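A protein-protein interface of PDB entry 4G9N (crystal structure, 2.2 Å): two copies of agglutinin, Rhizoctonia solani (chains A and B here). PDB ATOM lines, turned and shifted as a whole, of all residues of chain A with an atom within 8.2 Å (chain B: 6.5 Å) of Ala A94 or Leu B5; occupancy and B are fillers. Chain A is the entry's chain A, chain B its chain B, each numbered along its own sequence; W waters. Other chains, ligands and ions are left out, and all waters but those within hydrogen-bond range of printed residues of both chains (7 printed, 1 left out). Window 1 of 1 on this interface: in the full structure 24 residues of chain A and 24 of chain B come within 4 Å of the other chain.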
ATOM      1  N   ALA A   1     -17.999   0.589  16.459  1.00  0.00           N
ATOM      2  CA  ALA A   1     -18.409  -0.284  15.367  1.00  0.00           C
ATOM      3  C   ALA A   1     -18.631   0.545  14.102  1.00  0.00           C
ATOM      4  O   ALA A   1     -19.017   1.719  14.198  1.00  0.00           O
ATOM      5  CB  ALA A   1     -19.674  -1.055  15.752  1.00  0.00           C
ATOM      6  N   PRO A   2     -18.369  -0.056  12.919  1.00  0.00           N
ATOM      7  CA  PRO A   2     -18.404   0.648  11.624  1.00  0.00           C
ATOM      8  C   PRO A   2     -19.817   0.934  11.126  1.00  0.00           C
ATOM      9  O   PRO A   2     -20.455   0.069  10.534  1.00  0.00           O
ATOM     10  CB  PRO A   2     -17.712  -0.328  10.656  1.00  0.00           C
ATOM     11  CG  PRO A   2     -17.052  -1.354  11.516  1.00  0.00           C
ATOM     12  CD  PRO A   2     -17.860  -1.431  12.776  1.00  0.00           C
ATOM     13  N   ILE A   3     -20.287   2.155  11.338  1.00  0.00           N
ATOM     14  CA  ILE A   3     -21.621   2.527  10.903  1.00  0.00           C
ATOM     15  C   ILE A   3     -21.695   2.684   9.388  1.00  0.00           C
ATOM     16  O   ILE A   3     -21.078   3.586   8.801  1.00  0.00           O
ATOM     17  CB  ILE A   3     -22.068   3.810  11.578  1.00  0.00           C
ATOM     18  CG1 ILE A   3     -22.147   3.580  13.090  1.00  0.00           C
ATOM     19  CG2 ILE A   3     -23.409   4.263  11.002  1.00  0.00           C
ATOM     20  CD1 ILE A   3     -22.354   4.835  13.874  1.00  0.00           C
ATOM     21  N   SER A   4     -22.450   1.792   8.759  1.00  0.00           N
ATOM     22  CA  SER A   4     -22.672   1.864   7.322  1.00  0.00           C
ATOM     23  C   SER A   4     -24.157   1.914   7.000  1.00  0.00           C
ATOM     24  O   SER A   4     -24.988   1.424   7.770  1.00  0.00           O
ATOM     25  CB  SER A   4     -22.018   0.671   6.608  1.00  0.00           C
ATOM     26  OG  SER A   4     -22.590  -0.549   7.042  1.00  0.00           O
ATOM     27  N   LEU A   5     -24.482   2.521   5.862  1.00  0.00           N
ATOM     28  CA  LEU A   5     -25.831   2.481   5.325  1.00  0.00           C
ATOM     29  C   LEU A   5     -25.755   1.671   4.032  1.00  0.00           C
ATOM     30  O   LEU A   5     -25.537   2.224   2.968  1.00  0.00           O
ATOM     31  CB  LEU A   5     -26.327   3.901   5.045  1.00  0.00           C
ATOM     32  CG  LEU A   5     -27.829   4.158   4.966  1.00  0.00           C
ATOM     33  CD1 LEU A   5     -28.520   3.863   6.294  1.00  0.00           C
ATOM     34  CD2 LEU A   5     -28.063   5.597   4.575  1.00  0.00           C
ATOM     35  N   ASP A  91     -29.843  12.121  -2.745  1.00  0.00           N
ATOM     36  CA  ASP A  91     -28.649  12.095  -1.915  1.00  0.00           C
ATOM     37  C   ASP A  91     -29.078  11.832  -0.478  1.00  0.00           C
ATOM     38  O   ASP A  91     -30.049  12.433  -0.010  1.00  0.00           O
ATOM     39  CB  ASP A  91     -27.914  13.434  -1.989  1.00  0.00           C
ATOM     40  CG  ASP A  91     -26.858  13.474  -3.081  1.00  0.00           C
ATOM     41  OD1 ASP A  91     -26.308  12.411  -3.439  1.00  0.00           O
ATOM     42  OD2 ASP A  91     -26.551  14.583  -3.573  1.00  0.00           O
ATOM     43  N   ILE A  92     -28.383  10.930   0.217  1.00  0.00           N
ATOM     44  CA  ILE A  92     -28.673  10.663   1.633  1.00  0.00           C
ATOM     45  C   ILE A  92     -27.658  11.387   2.515  1.00  0.00           C
ATOM     46  O   ILE A  92     -26.484  11.033   2.540  1.00  0.00           O
ATOM     47  CB  ILE A  92     -28.628   9.151   1.983  1.00  0.00           C
ATOM     48  CG1 ILE A  92     -29.485   8.326   1.014  1.00  0.00           C
ATOM     49  CG2 ILE A  92     -29.071   8.925   3.442  1.00  0.00           C
ATOM     50  CD1 ILE A  92     -30.912   8.829   0.857  1.00  0.00           C
ATOM     51  N   VAL A  93     -28.112  12.404   3.232  1.00  0.00           N
ATOM     52  CA  VAL A  93     -27.205  13.273   3.977  1.00  0.00           C
ATOM     53  C   VAL A  93     -27.433  13.111   5.474  1.00  0.00           C
ATOM     54  O   VAL A  93     -28.560  13.204   5.948  1.00  0.00           O
ATOM     55  CB  VAL A  93     -27.410  14.764   3.601  1.00  0.00           C
ATOM     56  CG1 VAL A  93     -26.367  15.635   4.280  1.00  0.00           C
ATOM     57  CG2 VAL A  93     -27.368  14.948   2.083  1.00  0.00           C
ATOM     58  N   ALA A  94     -26.359  12.874   6.215  1.00  0.00           N
ATOM     59  CA  ALA A  94     -26.457  12.642   7.653  1.00  0.00           C
ATOM     60  C   ALA A  94     -26.937  13.897   8.367  1.00  0.00           C
ATOM     61  O   ALA A  94     -26.382  14.986   8.178  1.00  0.00           O
ATOM     62  CB  ALA A  94     -25.114  12.181   8.217  1.00  0.00           C
ATOM     63  N   ALA A  95     -27.981  13.732   9.172  1.00  0.00           N
ATOM     64  CA  ALA A  95     -28.586  14.822   9.916  1.00  0.00           C
ATOM     65  C   ALA A  95     -28.421  14.600  11.429  1.00  0.00           C
ATOM     66  O   ALA A  95     -28.056  13.505  11.872  1.00  0.00           O
ATOM     67  CB  ALA A  95     -30.055  14.952   9.531  1.00  0.00           C
ATOM     68  N   ASP A  96     -28.683  15.639  12.219  1.00  0.00           N
ATOM     69  CA  ASP A  96     -28.487  15.564  13.668  1.00  0.00           C
ATOM     70  C   ASP A  96     -29.361  14.472  14.287  1.00  0.00           C
ATOM     71  O   ASP A  96     -29.036  13.923  15.341  1.00  0.00           O
ATOM     72  CB  ASP A  96     -28.768  16.924  14.329  1.00  0.00           C
ATOM     73  CG  ASP A  96     -30.244  17.290  14.310  1.00  0.00           C
ATOM     74  OD1 ASP A  96     -30.790  17.538  13.211  1.00  0.00           O
ATOM     75  OD2 ASP A  96     -30.854  17.339  15.396  1.00  0.00           O
ATOM     76  N   LYS A  97     -30.477  14.184  13.620  1.00  0.00           N
ATOM     77  CA  LYS A  97     -31.288  12.999  13.870  1.00  0.00           C
ATOM     78  C   LYS A  97     -31.644  12.394  12.517  1.00  0.00           C
ATOM     79  O   LYS A  97     -32.077  13.108  11.615  1.00  0.00           O
ATOM     80  CB  LYS A  97     -32.568  13.378  14.594  1.00  0.00           C
ATOM     81  CG  LYS A  97     -32.344  14.218  15.829  1.00  0.00           C
ATOM     82  CD  LYS A  97     -33.655  14.803  16.315  1.00  0.00           C
ATOM     83  CE  LYS A  97     -33.475  15.543  17.617  1.00  0.00           C
ATOM     84  NZ  LYS A  97     -34.783  16.115  18.032  1.00  0.00           N
ATOM     85  N   GLY A  98     -31.450  11.090  12.367  1.00  0.00           N
ATOM     86  CA  GLY A  98     -31.728  10.432  11.109  1.00  0.00           C
ATOM     87  C   GLY A  98     -30.959  11.006   9.931  1.00  0.00           C
ATOM     88  O   GLY A  98     -29.857  11.512  10.091  1.00  0.00           O
ATOM     89  N   PHE A  99     -31.547  10.914   8.744  1.00  0.00           N
ATOM     90  CA  PHE A  99     -30.923  11.407   7.523  1.00  0.00           C
ATOM     91  C   PHE A  99     -31.879  12.316   6.754  1.00  0.00           C
ATOM     92  O   PHE A  99     -33.092  12.099   6.752  1.00  0.00           O
ATOM     93  CB  PHE A  99     -30.520  10.229   6.613  1.00  0.00           C
ATOM     94  CG  PHE A  99     -29.452   9.337   7.194  1.00  0.00           C
ATOM     95  CD1 PHE A  99     -29.769   8.371   8.134  1.00  0.00           C
ATOM     96  CD2 PHE A  99     -28.131   9.457   6.787  1.00  0.00           C
ATOM     97  CE1 PHE A  99     -28.784   7.543   8.666  1.00  0.00           C
ATOM     98  CE2 PHE A  99     -27.143   8.635   7.314  1.00  0.00           C
ATOM     99  CZ  PHE A  99     -27.469   7.681   8.253  1.00  0.00           C
ATOM    100  N   ALA A 100     -31.329  13.331   6.095  1.00  0.00           N
ATOM    101  CA  ALA A 100     -32.073  14.075   5.087  1.00  0.00           C
ATOM    102  C   ALA A 100     -31.973  13.397   3.720  1.00  0.00           C
ATOM    103  O   ALA A 100     -30.937  12.831   3.359  1.00  0.00           O
ATOM    104  CB  ALA A 100     -31.575  15.517   5.001  1.00  0.00           C
ATOM    105  N   ILE A 101     -33.058  13.484   2.957  1.00  0.00           N
ATOM    106  CA  ILE A 101     -33.124  12.903   1.622  1.00  0.00           C
ATOM    107  C   ILE A 101     -33.292  14.010   0.578  1.00  0.00           C
ATOM    108  O   ILE A 101     -34.401  14.478   0.347  1.00  0.00           O
ATOM    109  CB  ILE A 101     -34.292  11.892   1.529  1.00  0.00           C
ATOM    110  CG1 ILE A 101     -34.206  10.890   2.687  1.00  0.00           C
ATOM    111  CG2 ILE A 101     -34.287  11.177   0.186  1.00  0.00           C
ATOM    112  CD1 ILE A 101     -35.330   9.860   2.720  1.00  0.00           C
ATOM    113  N   GLU A 102     -32.183  14.447  -0.024  1.00  0.00           N
ATOM    114  CA  GLU A 102     -32.219  15.555  -0.978  1.00  0.00           C
ATOM    115  C   GLU A 102     -32.498  15.024  -2.365  1.00  0.00           C
ATOM    116  O   GLU A 102     -32.131  13.888  -2.686  1.00  0.00           O
ATOM    117  CB  GLU A 102     -30.881  16.323  -1.045  1.00  0.00           C
ATOM    118  CG  GLU A 102     -30.428  17.061   0.208  1.00  0.00           C
ATOM    119  CD  GLU A 102     -29.046  17.702   0.042  1.00  0.00           C
ATOM    120  OE1 GLU A 102     -28.401  17.498  -1.006  1.00  0.00           O
ATOM    121  OE2 GLU A 102     -28.602  18.415   0.962  1.00  0.00           O
ATOM    122  N   LYS A 136     -36.339  14.889   8.310  1.00  0.00           N
ATOM    123  CA  LYS A 136     -35.321  13.911   8.650  1.00  0.00           C
ATOM    124  C   LYS A 136     -35.960  12.548   8.785  1.00  0.00           C
ATOM    125  O   LYS A 136     -37.082  12.426   9.268  1.00  0.00           O
ATOM    126  CB  LYS A 136     -34.600  14.300   9.938  1.00  0.00           C
ATOM    127  CG  LYS A 136     -33.882  15.643   9.828  1.00  0.00           C
ATOM    128  CD  LYS A 136     -33.503  16.202  11.191  1.00  0.00           C
ATOM    129  CE  LYS A 136     -33.229  17.701  11.090  1.00  0.00           C
ATOM    130  NZ  LYS A 136     -33.155  18.358  12.430  1.00  0.00           N
ATOM    131  N   TRP A 137     -35.228  11.524   8.353  1.00  0.00           N
ATOM    132  CA  TRP A 137     -35.756  10.170   8.242  1.00  0.00           C
ATOM    133  C   TRP A 137     -34.821   9.155   8.873  1.00  0.00           C
ATOM    134  O   TRP A 137     -33.624   9.138   8.585  1.00  0.00           O
ATOM    135  CB  TRP A 137     -35.971   9.825   6.766  1.00  0.00           C
ATOM    136  CG  TRP A 137     -36.901  10.772   6.094  1.00  0.00           C
ATOM    137  CD1 TRP A 137     -36.577  11.945   5.471  1.00  0.00           C
ATOM    138  CD2 TRP A 137     -38.325  10.645   6.000  1.00  0.00           C
ATOM    139  NE1 TRP A 137     -37.713  12.547   4.977  1.00  0.00           N
ATOM    140  CE2 TRP A 137     -38.800  11.774   5.296  1.00  0.00           C
ATOM    141  CE3 TRP A 137     -39.240   9.683   6.433  1.00  0.00           C
ATOM    142  CZ2 TRP A 137     -40.152  11.968   5.021  1.00  0.00           C
ATOM    143  CZ3 TRP A 137     -40.581   9.876   6.161  1.00  0.00           C
ATOM    144  CH2 TRP A 137     -41.026  11.007   5.457  1.00  0.00           C
ATOM    145  N   ILE B   3     -30.438   2.533  11.737  1.00  0.00           N
ATOM    146  CA  ILE B   3     -29.050   2.876  11.487  1.00  0.00           C
ATOM    147  C   ILE B   3     -28.912   4.375  11.626  1.00  0.00           C
ATOM    148  O   ILE B   3     -29.595   5.142  10.945  1.00  0.00           O
ATOM    149  CB  ILE B   3     -28.590   2.450  10.093  1.00  0.00           C
ATOM    150  CG1 ILE B   3     -28.628   0.923   9.968  1.00  0.00           C
ATOM    151  CG2 ILE B   3     -27.191   2.987   9.819  1.00  0.00           C
ATOM    152  CD1 ILE B   3     -28.212   0.414   8.604  1.00  0.00           C
ATOM    153  N   SER B   4     -28.045   4.797  12.533  1.00  0.00           N
ATOM    154  CA  SER B   4     -27.837   6.215  12.733  1.00  0.00           C
ATOM    155  C   SER B   4     -26.349   6.515  12.767  1.00  0.00           C
ATOM    156  O   SER B   4     -25.541   5.659  13.120  1.00  0.00           O
ATOM    157  CB  SER B   4     -28.499   6.681  14.034  1.00  0.00           C
ATOM    158  OG  SER B   4     -27.787   6.183  15.150  1.00  0.00           O
ATOM    159  N   LEU B   5     -26.001   7.732  12.368  1.00  0.00           N
ATOM    160  CA  LEU B   5     -24.657   8.239  12.514  1.00  0.00           C
ATOM    161  C   LEU B   5     -24.723   9.360  13.538  1.00  0.00           C
ATOM    162  O   LEU B   5     -24.867  10.521  13.172  1.00  0.00           O
ATOM    163  CB  LEU B   5     -24.159   8.781  11.181  1.00  0.00           C
ATOM    164  CG  LEU B   5     -22.670   9.138  11.127  1.00  0.00           C
ATOM    165  CD1 LEU B   5     -21.834   7.868  11.174  1.00  0.00           C
ATOM    166  CD2 LEU B   5     -22.357   9.972   9.892  1.00  0.00           C
ATOM    167  N   PRO B   6     -24.632   9.013  14.831  1.00  0.00           N
ATOM    168  CA  PRO B   6     -24.821  10.012  15.885  1.00  0.00           C
ATOM    169  C   PRO B   6     -23.605  10.897  16.013  1.00  0.00           C
ATOM    170  O   PRO B   6     -22.516  10.510  15.588  1.00  0.00           O
ATOM    171  CB  PRO B   6     -24.954   9.159  17.142  1.00  0.00           C
ATOM    172  CG  PRO B   6     -24.109   7.968  16.857  1.00  0.00           C
ATOM    173  CD  PRO B   6     -24.282   7.691  15.383  1.00  0.00           C
ATOM    174  N   ALA B   7     -23.788  12.082  16.578  1.00  0.00           N
ATOM    175  CA  ALA B   7     -22.648  12.894  16.958  1.00  0.00           C
ATOM    176  C   ALA B   7     -21.841  12.082  17.972  1.00  0.00           C
ATOM    177  O   ALA B   7     -22.402  11.404  18.833  1.00  0.00           O
ATOM    178  CB  ALA B   7     -23.102  14.226  17.550  1.00  0.00           C
ATOM    179  N   TYR B  10     -15.103   9.427  16.250  1.00  0.00           N
ATOM    180  CA  TYR B  10     -14.976   8.416  15.212  1.00  0.00           C
ATOM    181  C   TYR B  10     -13.547   8.155  14.795  1.00  0.00           C
ATOM    182  O   TYR B  10     -12.729   9.072  14.728  1.00  0.00           O
ATOM    183  CB  TYR B  10     -15.754   8.848  13.969  1.00  0.00           C
ATOM    184  CG  TYR B  10     -17.249   8.741  14.113  1.00  0.00           C
ATOM    185  CD1 TYR B  10     -17.995   9.792  14.641  1.00  0.00           C
ATOM    186  CD2 TYR B  10     -17.917   7.589  13.720  1.00  0.00           C
ATOM    187  CE1 TYR B  10     -19.366   9.696  14.772  1.00  0.00           C
ATOM    188  CE2 TYR B  10     -19.289   7.486  13.839  1.00  0.00           C
ATOM    189  CZ  TYR B  10     -20.006   8.538  14.374  1.00  0.00           C
ATOM    190  OH  TYR B  10     -21.360   8.420  14.499  1.00  0.00           O
ATOM    191  N   LEU B  49     -17.469  14.182  15.581  1.00  0.00           N
ATOM    192  CA  LEU B  49     -18.488  14.612  14.627  1.00  0.00           C
ATOM    193  C   LEU B  49     -19.561  15.383  15.375  1.00  0.00           C
ATOM    194  O   LEU B  49     -20.139  14.867  16.318  1.00  0.00           O
ATOM    195  CB  LEU B  49     -19.126  13.391  13.962  1.00  0.00           C
ATOM    196  CG  LEU B  49     -20.302  13.603  13.007  1.00  0.00           C
ATOM    197  CD1 LEU B  49     -19.867  14.443  11.814  1.00  0.00           C
ATOM    198  CD2 LEU B  49     -20.835  12.261  12.544  1.00  0.00           C
ATOM    199  N   TRP B  51     -22.897  18.372  14.883  1.00  0.00           N
ATOM    200  CA  TRP B  51     -23.718  19.221  14.042  1.00  0.00           C
ATOM    201  C   TRP B  51     -23.645  20.655  14.542  1.00  0.00           C
ATOM    202  O   TRP B  51     -23.587  20.897  15.742  1.00  0.00           O
ATOM    203  CB  TRP B  51     -25.156  18.693  13.948  1.00  0.00           C
ATOM    204  CG  TRP B  51     -25.282  17.655  12.858  1.00  0.00           C
ATOM    205  CD1 TRP B  51     -25.687  17.864  11.578  1.00  0.00           C
ATOM    206  CD2 TRP B  51     -24.955  16.260  12.953  1.00  0.00           C
ATOM    207  NE1 TRP B  51     -25.650  16.691  10.868  1.00  0.00           N
ATOM    208  CE2 TRP B  51     -25.212  15.688  11.692  1.00  0.00           C
ATOM    209  CE3 TRP B  51     -24.483  15.440  13.986  1.00  0.00           C
ATOM    210  CZ2 TRP B  51     -24.999  14.330  11.428  1.00  0.00           C
ATOM    211  CZ3 TRP B  51     -24.279  14.094  13.724  1.00  0.00           C
ATOM    212  CH2 TRP B  51     -24.534  13.554  12.453  1.00  0.00           C
ATOM    213  N   ASN B  56     -27.773  20.657   7.757  1.00  0.00           N
ATOM    214  CA  ASN B  56     -27.251  19.356   8.150  1.00  0.00           C
ATOM    215  C   ASN B  56     -25.725  19.415   8.284  1.00  0.00           C
ATOM    216  O   ASN B  56     -25.049  18.391   8.358  1.00  0.00           O
ATOM    217  CB  ASN B  56     -27.645  18.294   7.114  1.00  0.00           C
ATOM    218  CG  ASN B  56     -29.154  18.263   6.832  1.00  0.00           C
ATOM    219  OD1 ASN B  56     -29.581  18.373   5.679  1.00  0.00           O
ATOM    220  ND2 ASN B  56     -29.960  18.111   7.879  1.00  0.00           N
ATOM    221  N   GLN B  57     -25.187  20.625   8.318  1.00  0.00           N
ATOM    222  CA  GLN B  57     -23.744  20.822   8.333  1.00  0.00           C
ATOM    223  C   GLN B  57     -23.120  20.372   9.647  1.00  0.00           C
ATOM    224  O   GLN B  57     -23.735  20.489  10.716  1.00  0.00           O
ATOM    225  CB  GLN B  57     -23.411  22.289   8.043  1.00  0.00           C
ATOM    226  CG  GLN B  57     -23.944  22.741   6.697  1.00  0.00           C
ATOM    227  CD  GLN B  57     -23.557  24.160   6.330  1.00  0.00           C
ATOM    228  OE1 GLN B  57     -22.736  24.805   6.992  1.00  0.00           O
ATOM    229  NE2 GLN B  57     -24.153  24.653   5.254  1.00  0.00           N
ATOM    230  N   VAL B  58     -21.904  19.841   9.558  1.00  0.00           N
ATOM    231  CA  VAL B  58     -21.185  19.352  10.727  1.00  0.00           C
ATOM    232  C   VAL B  58     -19.782  19.899  10.695  1.00  0.00           C
ATOM    233  O   VAL B  58     -19.372  20.496   9.699  1.00  0.00           O
ATOM    234  CB  VAL B  58     -21.072  17.806  10.758  1.00  0.00           C
ATOM    235  CG1 VAL B  58     -22.438  17.165  10.596  1.00  0.00           C
ATOM    236  CG2 VAL B  58     -20.080  17.293   9.684  1.00  0.00           C
ATOM    237  N   ASP B  91     -20.600  18.338   4.883  1.00  0.00           N
ATOM    238  CA  ASP B  91     -21.794  17.497   4.755  1.00  0.00           C
ATOM    239  C   ASP B  91     -21.343  16.030   4.679  1.00  0.00           C
ATOM    240  O   ASP B  91     -20.429  15.698   3.925  1.00  0.00           O
ATOM    241  CB  ASP B  91     -22.582  17.829   3.485  1.00  0.00           C
ATOM    242  CG  ASP B  91     -23.523  19.021   3.643  1.00  0.00           C
ATOM    243  OD1 ASP B  91     -24.104  19.225   4.738  1.00  0.00           O
ATOM    244  OD2 ASP B  91     -23.707  19.743   2.635  1.00  0.00           O
ATOM    245  N   ILE B  92     -21.976  15.156   5.459  1.00  0.00           N
ATOM    246  CA  ILE B  92     -21.664  13.726   5.420  1.00  0.00           C
ATOM    247  C   ILE B  92     -22.710  12.990   4.572  1.00  0.00           C
ATOM    248  O   ILE B  92     -23.884  12.887   4.953  1.00  0.00           O
ATOM    249  CB  ILE B  92     -21.582  13.131   6.843  1.00  0.00           C
ATOM    250  CG1 ILE B  92     -20.723  14.020   7.752  1.00  0.00           C
ATOM    251  CG2 ILE B  92     -21.046  11.707   6.815  1.00  0.00           C
ATOM    252  CD1 ILE B  92     -19.297  14.189   7.285  1.00  0.00           C
ATOM    253  N   VAL B  93     -22.281  12.497   3.415  1.00  0.00           N
ATOM    254  CA  VAL B  93     -23.193  11.935   2.419  1.00  0.00           C
ATOM    255  C   VAL B  93     -22.997  10.419   2.261  1.00  0.00           C
ATOM    256  O   VAL B  93     -21.867   9.947   2.119  1.00  0.00           O
ATOM    257  CB  VAL B  93     -22.971  12.613   1.042  1.00  0.00           C
ATOM    258  CG1 VAL B  93     -23.962  12.086   0.002  1.00  0.00           C
ATOM    259  CG2 VAL B  93     -23.062  14.129   1.176  1.00  0.00           C
ATOM    260  N   ALA B  94     -24.087   9.653   2.277  1.00  0.00           N
ATOM    261  CA  ALA B  94     -23.971   8.203   2.139  1.00  0.00           C
ATOM    262  C   ALA B  94     -23.477   7.796   0.757  1.00  0.00           C
ATOM    263  O   ALA B  94     -24.047   8.199  -0.266  1.00  0.00           O
ATOM    264  CB  ALA B  94     -25.291   7.512   2.458  1.00  0.00           C
ATOM    265  N   PHE B  99     -18.961   6.783   3.642  1.00  0.00           N
ATOM    266  CA  PHE B  99     -19.565   8.096   3.398  1.00  0.00           C
ATOM    267  C   PHE B  99     -18.606   9.030   2.684  1.00  0.00           C
ATOM    268  O   PHE B  99     -17.385   8.946   2.873  1.00  0.00           O
ATOM    269  CB  PHE B  99     -19.969   8.765   4.718  1.00  0.00           C
ATOM    270  CG  PHE B  99     -21.054   8.046   5.466  1.00  0.00           C
ATOM    271  CD1 PHE B  99     -20.753   6.985   6.308  1.00  0.00           C
ATOM    272  CD2 PHE B  99     -22.375   8.440   5.341  1.00  0.00           C
ATOM    273  CE1 PHE B  99     -21.750   6.315   6.999  1.00  0.00           C
ATOM    274  CE2 PHE B  99     -23.377   7.770   6.028  1.00  0.00           C
ATOM    275  CZ  PHE B  99     -23.060   6.708   6.865  1.00  0.00           C
ATOM    276  N   PHE B 139     -17.027   5.369   8.790  1.00  0.00           N
ATOM    277  CA  PHE B 139     -17.143   5.965  10.108  1.00  0.00           C
ATOM    278  C   PHE B 139     -17.239   4.867  11.169  1.00  0.00           C
ATOM    279  O   PHE B 139     -18.248   4.154  11.272  1.00  0.00           O
ATOM    280  CB  PHE B 139     -18.352   6.890  10.162  1.00  0.00           C
ATOM    281  CG  PHE B 139     -18.131   8.209   9.475  1.00  0.00           C
ATOM    282  CD1 PHE B 139     -17.811   8.261   8.131  1.00  0.00           C
ATOM    283  CD2 PHE B 139     -18.246   9.400  10.183  1.00  0.00           C
ATOM    284  CE1 PHE B 139     -17.608   9.463   7.501  1.00  0.00           C
ATOM    285  CE2 PHE B 139     -18.043  10.609   9.558  1.00  0.00           C
ATOM    286  CZ  PHE B 139     -17.731  10.640   8.215  1.00  0.00           C
HETATM  287  O   HOH W   1     -28.014  18.936   3.629  1.00  0.00           O
HETATM  288  O   HOH W   2     -26.360   9.392  -1.029  1.00  0.00           O
HETATM  289  O   HOH W   3     -19.010   3.858   7.402  1.00  0.00           O
HETATM  290  O   HOH W   4     -24.220  15.942   7.153  1.00  0.00           O
HETATM  291  O   HOH W   5     -27.681  10.064  11.826  1.00  0.00           O
HETATM  292  O   HOH W   6     -29.460  18.580  10.919  1.00  0.00           O
HETATM  293  O   HOH W   7     -26.441  12.884  16.627  1.00  0.00           O
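The backbone NH of Ile A3 sits at hydrogen-bond distance from the backbone carbonyl oxygen of Phe B139, at 2.9 Å.
N of Ala B94 sits at hydrogen-bond distance from O of Ile A92 (2.8 Å).
NE1 of Trp B51 lies within hydrogen-bond range of O of Ala A94, at 3.3 Å.
The backbone NH of Ala A94 is in hydrogen-bond range of the backbone carbonyl oxygen of Ile B92, 2.8 Å away.
N of Asp A96 sits close to NE1 of Trp B51, 3.5 Å away.
O of Val A93 is in hydrogen-bond range of N of Ala A100.
NZ of Lys A136 lies within salt-bridge range of OD1 of Asp A96 (2.6 Å).
O of Phe A99 is in hydrogen-bond range of N of Trp A137.
The backbone carbonyl oxygen (O) of Pro B6 is in hydrogen-bond range of the side-chain hydroxyl (OH) of Tyr B10, 2.6 Å away.
The backbone carbonyl oxygen (O) of Asn B56 is in hydrogen-bond range of the indole nitrogen (NE1) of Trp B51 (3.1 Å).
Among the printed residues, merely in contact across the chains: Ala A95 with Trp B51 (3.2 Å), Ile A3 with Ser B4 (3.3 Å), Ile A3 with Phe B99 (3.3 Å), Ser A4 with Ile B3 (3.4 Å), Phe A99 with Ile B3 (3.4 Å), Ile A92 with Val B93 (3.4 Å), Val A93 with Ile B92 (3.5 Å), Pro A2 with Phe B139 (3.5 Å), Ala A100 with Asn B56 (3.5 Å), Ala A95 with Asn B56 (3.6 Å), Ala A94 with Asn B56 (3.7 Å), Ile A3 with Pro B6 (3.8 Å), Ile A3 with Tyr B10 (3.8 Å), Leu A5 with Ile B3 (3.9 Å), Ala A1 with Phe B139 (3.9 Å), Ala A94 with Leu B5 (3.9 Å), Ile A3 with Leu B5 (3.9 Å) and Leu A5 with Ala B94 (3.98 Å).
Ala A94 touches just these residues of chain B: Leu B5, Trp B51, Asn B56 and Ile B92.
Of chain A, only Ile A3 comes within 4 Å of Ser B4.
Leu B5 touches just these residues of chain A: Ile A3 (3.9 Å) and Ala A94 (3.9 Å).
Of chain A, only Ile A3 comes within 4 Å of Pro B6.
Printed residues of chain A within 4 Å of Ile B92: Val A93 and Ala A94.
Of the printed residues of chain A, Val B93 touches Ile A92 (3.4 Å).
Of the printed residues of chain A, Ala B94 touches Leu A5 (3.98 Å) and Ile A92 (2.8 Å).
Of the printed residues of chain A, Phe B139 touches Ala A1, Pro A2 and Ile A3.
The nearest residue of chain B that does not touch Ala A94 is Val B93 (5.0 Å).
The nearest printed residue of chain B that does not touch Pro A2 is Phe B99 (7.1 Å).
Hydrophobic or aromatic side chains of chain A within 4 Å of the printed part of chain B: Ile A3, Leu A5, Ile A92, Val A93, Ala A94, Ala A95, Phe A99 and Ala A100.
Ile A3 touches Ser B4, and with the chains exchanged Ser A4 touches Ile B3.
Ile A3 touches Leu B5, and with the chains exchanged Leu A5 touches Ile B3.
Ile A92 touches Val B93, and with the chains exchanged Val A93 touches Ile B92.
Ile A92 touches Ala B94, and with the chains exchanged Ala A94 touches Ile B92.
Of the 23 pairs that touch across the chains among the printed residues, 12 have their exchanged pair printed and touching as well.
Water W3 lies within hydrogen-bond range of O of Ile A3 and N of Phe B139.
Water W1 lies within hydrogen-bond range of the side-chain amide oxygen of Asn B56 (2.6 Å) and the side-chain carboxylate of Glu A102 (2.8 Å).
Water W2 bridges the backbone carbonyl oxygen of Ala B94 (2.7 Å) and the backbone NH of Ile A92 (2.8 Å).
Water W7 lies within hydrogen-bond range of N of Ala B7 (2.8 Å) and O of Asp A96 (3.1 Å).
Water W6 lies within hydrogen-bond range of the side-chain carboxylate (OD1) of Asp A96 (2.8 Å) and the side-chain amide nitrogen (ND2) of Asn B56 (3.1 Å).
Water W5 lies within hydrogen-bond range of N of Leu B5, O of Gly A98 and O of Ala A95.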
